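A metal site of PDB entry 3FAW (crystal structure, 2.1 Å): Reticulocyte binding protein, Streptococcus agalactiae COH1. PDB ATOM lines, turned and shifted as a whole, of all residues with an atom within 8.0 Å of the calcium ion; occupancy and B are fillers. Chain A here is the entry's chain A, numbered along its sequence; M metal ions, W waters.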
ATOM      1  N   TYR A 163     -34.277 -29.715  -7.472  1.00  0.00           N
ATOM      2  CA  TYR A 163     -34.777 -29.982  -8.815  1.00  0.00           C
ATOM      3  C   TYR A 163     -33.783 -30.816  -9.621  1.00  0.00           C
ATOM      4  O   TYR A 163     -32.573 -30.615  -9.531  1.00  0.00           O
ATOM      5  CB  TYR A 163     -35.067 -28.680  -9.564  1.00  0.00           C
ATOM      6  CG  TYR A 163     -36.019 -27.747  -8.839  1.00  0.00           C
ATOM      7  CD1 TYR A 163     -37.390 -27.779  -9.111  1.00  0.00           C
ATOM      8  CD2 TYR A 163     -35.555 -26.846  -7.896  1.00  0.00           C
ATOM      9  CE1 TYR A 163     -38.259 -26.921  -8.451  1.00  0.00           C
ATOM     10  CE2 TYR A 163     -36.420 -25.985  -7.227  1.00  0.00           C
ATOM     11  CZ  TYR A 163     -37.777 -26.030  -7.512  1.00  0.00           C
ATOM     12  OH  TYR A 163     -38.641 -25.185  -6.849  1.00  0.00           O
ATOM     13  N   ASP A 164     -34.324 -31.734 -10.428  1.00  0.00           N
ATOM     14  CA  ASP A 164     -33.518 -32.637 -11.262  1.00  0.00           C
ATOM     15  C   ASP A 164     -32.530 -31.881 -12.146  1.00  0.00           C
ATOM     16  O   ASP A 164     -32.902 -30.978 -12.893  1.00  0.00           O
ATOM     17  CB  ASP A 164     -34.442 -33.506 -12.125  1.00  0.00           C
ATOM     18  CG  ASP A 164     -33.693 -34.548 -12.949  1.00  0.00           C
ATOM     19  OD1 ASP A 164     -32.449 -34.589 -12.918  1.00  0.00           O
ATOM     20  OD2 ASP A 164     -34.372 -35.345 -13.628  1.00  0.00           O
ATOM     21  N   LYS A 165     -31.266 -32.280 -12.076  1.00  0.00           N
ATOM     22  CA  LYS A 165     -30.195 -31.720 -12.908  1.00  0.00           C
ATOM     23  C   LYS A 165     -30.498 -31.798 -14.410  1.00  0.00           C
ATOM     24  O   LYS A 165     -30.171 -30.870 -15.158  1.00  0.00           O
ATOM     25  CB  LYS A 165     -28.866 -32.426 -12.609  1.00  0.00           C
ATOM     26  CG  LYS A 165     -28.852 -33.927 -12.876  1.00  0.00           C
ATOM     27  CD  LYS A 165     -27.522 -34.563 -12.488  1.00  0.00           C
ATOM     28  CE  LYS A 165     -27.515 -36.059 -12.799  1.00  0.00           C
ATOM     29  NZ  LYS A 165     -26.229 -36.710 -12.411  1.00  0.00           N
ATOM     30  N   ASP A 166     -31.114 -32.891 -14.841  1.00  0.00           N
ATOM     31  CA  ASP A 166     -31.432 -33.125 -16.255  1.00  0.00           C
ATOM     32  C   ASP A 166     -32.848 -32.693 -16.645  1.00  0.00           C
ATOM     33  O   ASP A 166     -33.269 -32.895 -17.783  1.00  0.00           O
ATOM     34  CB  ASP A 166     -31.227 -34.607 -16.614  1.00  0.00           C
ATOM     35  CG  ASP A 166     -29.766 -35.006 -16.621  1.00  0.00           C
ATOM     36  OD1 ASP A 166     -28.894 -34.124 -16.817  1.00  0.00           O
ATOM     37  OD2 ASP A 166     -29.474 -36.208 -16.443  1.00  0.00           O
ATOM     38  N   ASN A 167     -33.583 -32.080 -15.714  1.00  0.00           N
ATOM     39  CA  ASN A 167     -34.940 -31.579 -15.959  1.00  0.00           C
ATOM     40  C   ASN A 167     -35.286 -30.594 -14.838  1.00  0.00           C
ATOM     41  O   ASN A 167     -35.895 -30.971 -13.830  1.00  0.00           O
ATOM     42  CB  ASN A 167     -35.929 -32.752 -16.017  1.00  0.00           C
ATOM     43  CG  ASN A 167     -37.367 -32.310 -16.312  1.00  0.00           C
ATOM     44  OD1 ASN A 167     -37.688 -31.112 -16.333  1.00  0.00           O
ATOM     45  ND2 ASN A 167     -38.239 -33.287 -16.545  1.00  0.00           N
ATOM     46  N   GLN A 168     -34.909 -29.339 -15.014  1.00  0.00           N
ATOM     47  CA  GLN A 168     -34.967 -28.354 -13.928  1.00  0.00           C
ATOM     48  C   GLN A 168     -36.368 -28.060 -13.373  1.00  0.00           C
ATOM     49  O   GLN A 168     -36.487 -27.519 -12.278  1.00  0.00           O
ATOM     50  CB  GLN A 168     -34.294 -27.033 -14.342  1.00  0.00           C
ATOM     51  CG  GLN A 168     -35.036 -26.247 -15.410  1.00  0.00           C
ATOM     52  CD  GLN A 168     -34.712 -24.774 -15.378  1.00  0.00           C
ATOM     53  OE1 GLN A 168     -34.958 -24.102 -14.365  1.00  0.00           O
ATOM     54  NE2 GLN A 168     -34.174 -24.247 -16.472  1.00  0.00           N
ATOM     55  N   THR A 199     -24.039 -33.070  -7.628  1.00  0.00           N
ATOM     56  CA  THR A 199     -23.424 -32.222  -8.641  1.00  0.00           C
ATOM     57  C   THR A 199     -24.414 -31.984  -9.797  1.00  0.00           C
ATOM     58  O   THR A 199     -24.997 -32.926 -10.334  1.00  0.00           O
ATOM     59  CB  THR A 199     -22.109 -32.845  -9.181  1.00  0.00           C
ATOM     60  OG1 THR A 199     -21.244 -33.174  -8.082  1.00  0.00           O
ATOM     61  CG2 THR A 199     -21.388 -31.880 -10.127  1.00  0.00           C
ATOM     62  N   GLY A 200     -24.617 -30.714 -10.144  1.00  0.00           N
ATOM     63  CA  GLY A 200     -25.509 -30.349 -11.244  1.00  0.00           C
ATOM     64  C   GLY A 200     -26.984 -30.177 -10.879  1.00  0.00           C
ATOM     65  O   GLY A 200     -27.745 -29.618 -11.666  1.00  0.00           O
ATOM     66  N   TYR A 201     -27.394 -30.653  -9.706  1.00  0.00           N
ATOM     67  CA  TYR A 201     -28.784 -30.466  -9.256  1.00  0.00           C
ATOM     68  C   TYR A 201     -29.042 -29.010  -8.901  1.00  0.00           C
ATOM     69  O   TYR A 201     -28.108 -28.260  -8.575  1.00  0.00           O
ATOM     70  CB  TYR A 201     -29.107 -31.380  -8.066  1.00  0.00           C
ATOM     71  CG  TYR A 201     -29.451 -32.809  -8.441  1.00  0.00           C
ATOM     72  CD1 TYR A 201     -28.451 -33.744  -8.691  1.00  0.00           C
ATOM     73  CD2 TYR A 201     -30.779 -33.221  -8.552  1.00  0.00           C
ATOM     74  CE1 TYR A 201     -28.759 -35.060  -9.048  1.00  0.00           C
ATOM     75  CE2 TYR A 201     -31.096 -34.537  -8.895  1.00  0.00           C
ATOM     76  CZ  TYR A 201     -30.084 -35.453  -9.144  1.00  0.00           C
ATOM     77  OH  TYR A 201     -30.399 -36.750  -9.471  1.00  0.00           O
ATOM     78  N   TYR A 202     -30.315 -28.611  -8.956  1.00  0.00           N
ATOM     79  CA  TYR A 202     -30.694 -27.213  -8.737  1.00  0.00           C
ATOM     80  C   TYR A 202     -31.547 -27.073  -7.475  1.00  0.00           C
ATOM     81  O   TYR A 202     -32.179 -28.033  -7.035  1.00  0.00           O
ATOM     82  CB  TYR A 202     -31.443 -26.669  -9.950  1.00  0.00           C
ATOM     83  CG  TYR A 202     -30.725 -26.879 -11.261  1.00  0.00           C
ATOM     84  CD1 TYR A 202     -31.213 -27.776 -12.219  1.00  0.00           C
ATOM     85  CD2 TYR A 202     -29.550 -26.191 -11.547  1.00  0.00           C
ATOM     86  CE1 TYR A 202     -30.551 -27.957 -13.428  1.00  0.00           C
ATOM     87  CE2 TYR A 202     -28.887 -26.372 -12.756  1.00  0.00           C
ATOM     88  CZ  TYR A 202     -29.390 -27.261 -13.688  1.00  0.00           C
ATOM     89  OH  TYR A 202     -28.728 -27.425 -14.891  1.00  0.00           O
ATOM     90  N   LEU A 224     -26.033 -21.588 -11.820  1.00  0.00           N
ATOM     91  CA  LEU A 224     -27.479 -21.603 -11.989  1.00  0.00           C
ATOM     92  C   LEU A 224     -27.925 -22.558 -13.091  1.00  0.00           C
ATOM     93  O   LEU A 224     -27.126 -22.945 -13.951  1.00  0.00           O
ATOM     94  CB  LEU A 224     -27.986 -20.204 -12.348  1.00  0.00           C
ATOM     95  CG  LEU A 224     -27.607 -18.999 -11.491  1.00  0.00           C
ATOM     96  CD1 LEU A 224     -27.949 -17.707 -12.238  1.00  0.00           C
ATOM     97  CD2 LEU A 224     -28.303 -19.028 -10.124  1.00  0.00           C
ATOM     98  N   ALA A 225     -29.205 -22.919 -13.058  1.00  0.00           N
ATOM     99  CA  ALA A 225     -29.857 -23.619 -14.171  1.00  0.00           C
ATOM    100  C   ALA A 225     -29.994 -22.671 -15.348  1.00  0.00           C
ATOM    101  O   ALA A 225     -30.077 -21.459 -15.163  1.00  0.00           O
ATOM    102  CB  ALA A 225     -31.222 -24.141 -13.740  1.00  0.00           C
ATOM    103  N   GLU A 226     -30.024 -23.223 -16.560  1.00  0.00           N
ATOM    104  CA  GLU A 226     -30.265 -22.421 -17.762  1.00  0.00           C
ATOM    105  C   GLU A 226     -31.503 -21.541 -17.536  1.00  0.00           C
ATOM    106  O   GLU A 226     -32.515 -22.011 -17.025  1.00  0.00           O
ATOM    107  CB  GLU A 226     -30.414 -23.297 -19.027  1.00  0.00           C
ATOM    108  CG  GLU A 226     -31.674 -24.177 -19.128  1.00  0.00           C
ATOM    109  CD  GLU A 226     -31.715 -25.342 -18.137  1.00  0.00           C
ATOM    110  OE1 GLU A 226     -30.677 -25.654 -17.514  1.00  0.00           O
ATOM    111  OE2 GLU A 226     -32.791 -25.954 -17.993  1.00  0.00           O
ATOM    112  N   ALA A 242     -27.497 -23.712  -8.479  1.00  0.00           N
ATOM    113  CA  ALA A 242     -26.954 -25.016  -8.859  1.00  0.00           C
ATOM    114  C   ALA A 242     -25.869 -25.451  -7.879  1.00  0.00           C
ATOM    115  O   ALA A 242     -25.129 -24.618  -7.359  1.00  0.00           O
ATOM    116  CB  ALA A 242     -26.391 -24.973 -10.280  1.00  0.00           C
ATOM    117  N   LYS A 361     -22.661 -24.540 -23.238  1.00  0.00           N
ATOM    118  CA  LYS A 361     -23.535 -25.549 -22.621  1.00  0.00           C
ATOM    119  C   LYS A 361     -24.255 -24.997 -21.385  1.00  0.00           C
ATOM    120  O   LYS A 361     -23.948 -25.399 -20.268  1.00  0.00           O
ATOM    121  CB  LYS A 361     -22.703 -26.783 -22.251  1.00  0.00           C
ATOM    122  CG  LYS A 361     -22.015 -27.449 -23.428  1.00  0.00           C
ATOM    123  CD  LYS A 361     -21.398 -28.774 -23.035  1.00  0.00           C
ATOM    124  CE  LYS A 361     -22.421 -29.909 -23.025  1.00  0.00           C
ATOM    125  NZ  LYS A 361     -21.787 -31.225 -22.742  1.00  0.00           N
ATOM    126  N   PRO A 362     -25.213 -24.073 -21.595  1.00  0.00           N
ATOM    127  CA  PRO A 362     -25.902 -23.431 -20.466  1.00  0.00           C
ATOM    128  C   PRO A 362     -26.661 -24.379 -19.522  1.00  0.00           C
ATOM    129  O   PRO A 362     -26.865 -24.049 -18.349  1.00  0.00           O
ATOM    130  CB  PRO A 362     -26.877 -22.450 -21.159  1.00  0.00           C
ATOM    131  CG  PRO A 362     -27.002 -22.935 -22.568  1.00  0.00           C
ATOM    132  CD  PRO A 362     -25.701 -23.593 -22.901  1.00  0.00           C
ATOM    133  N   LYS A 363     -27.065 -25.549 -20.022  1.00  0.00           N
ATOM    134  CA  LYS A 363     -27.753 -26.551 -19.211  1.00  0.00           C
ATOM    135  C   LYS A 363     -26.825 -27.319 -18.266  1.00  0.00           C
ATOM    136  O   LYS A 363     -27.303 -28.031 -17.382  1.00  0.00           O
ATOM    137  CB  LYS A 363     -28.540 -27.510 -20.121  1.00  0.00           C
ATOM    138  CG  LYS A 363     -29.763 -26.847 -20.761  1.00  0.00           C
ATOM    139  CD  LYS A 363     -30.173 -27.487 -22.077  1.00  0.00           C
ATOM    140  CE  LYS A 363     -30.771 -28.861 -21.888  1.00  0.00           C
ATOM    141  NZ  LYS A 363     -31.300 -29.421 -23.160  1.00  0.00           N
ATOM    142  N   ASP A 364     -25.510 -27.187 -18.452  1.00  0.00           N
ATOM    143  CA  ASP A 364     -24.508 -27.722 -17.531  1.00  0.00           C
ATOM    144  C   ASP A 364     -23.929 -26.568 -16.702  1.00  0.00           C
ATOM    145  O   ASP A 364     -23.164 -25.757 -17.214  1.00  0.00           O
ATOM    146  CB  ASP A 364     -23.396 -28.413 -18.350  1.00  0.00           C
ATOM    147  CG  ASP A 364     -22.275 -28.991 -17.473  1.00  0.00           C
ATOM    148  OD1 ASP A 364     -22.269 -28.784 -16.242  1.00  0.00           O
ATOM    149  OD2 ASP A 364     -21.390 -29.669 -18.051  1.00  0.00           O
ATOM    150  N   PRO A 365     -24.286 -26.484 -15.391  1.00  0.00           N
ATOM    151  CA  PRO A 365     -23.865 -25.329 -14.590  1.00  0.00           C
ATOM    152  C   PRO A 365     -22.362 -25.241 -14.298  1.00  0.00           C
ATOM    153  O   PRO A 365     -21.873 -24.180 -13.931  1.00  0.00           O
ATOM    154  CB  PRO A 365     -24.670 -25.499 -13.293  1.00  0.00           C
ATOM    155  CG  PRO A 365     -24.961 -26.939 -13.203  1.00  0.00           C
ATOM    156  CD  PRO A 365     -25.076 -27.450 -14.607  1.00  0.00           C
ATOM    157  N   SER A 366     -21.646 -26.342 -14.475  1.00  0.00           N
ATOM    158  CA  SER A 366     -20.199 -26.358 -14.273  1.00  0.00           C
ATOM    159  C   SER A 366     -19.438 -25.759 -15.466  1.00  0.00           C
ATOM    160  O   SER A 366     -18.342 -25.236 -15.310  1.00  0.00           O
ATOM    161  CB  SER A 366     -19.722 -27.794 -14.014  1.00  0.00           C
ATOM    162  OG  SER A 366     -20.190 -28.258 -12.754  1.00  0.00           O
HETATM  163 CA    CA M   1     -28.600 -29.561 -16.344  1.00  0.00          CA
HETATM  164  O   HOH W   1     -26.800 -31.234 -16.605  1.00  0.00           O
HETATM  165  O   HOH W   2     -27.267 -29.869 -14.226  1.00  0.00           O
HETATM  166  O   HOH W   3     -29.237 -30.809 -18.352  1.00  0.00           O
HETATM  167  O   HOH W   4     -30.729 -28.645 -16.901  1.00  0.00           O
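O of Tyr 202 sits at hydrogen-bond distance from N of Tyr 163.
Three residues have an atom within 4 Å of the calcium ion: Lys 165, Tyr 202 and Lys 363.
The calcium ion is bound by O of Lys 363, O of Lys 165, water W4, water W3, water W1, water W2 and OH of Tyr 202.
The calcium ion has seven donor atoms within binding distance.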
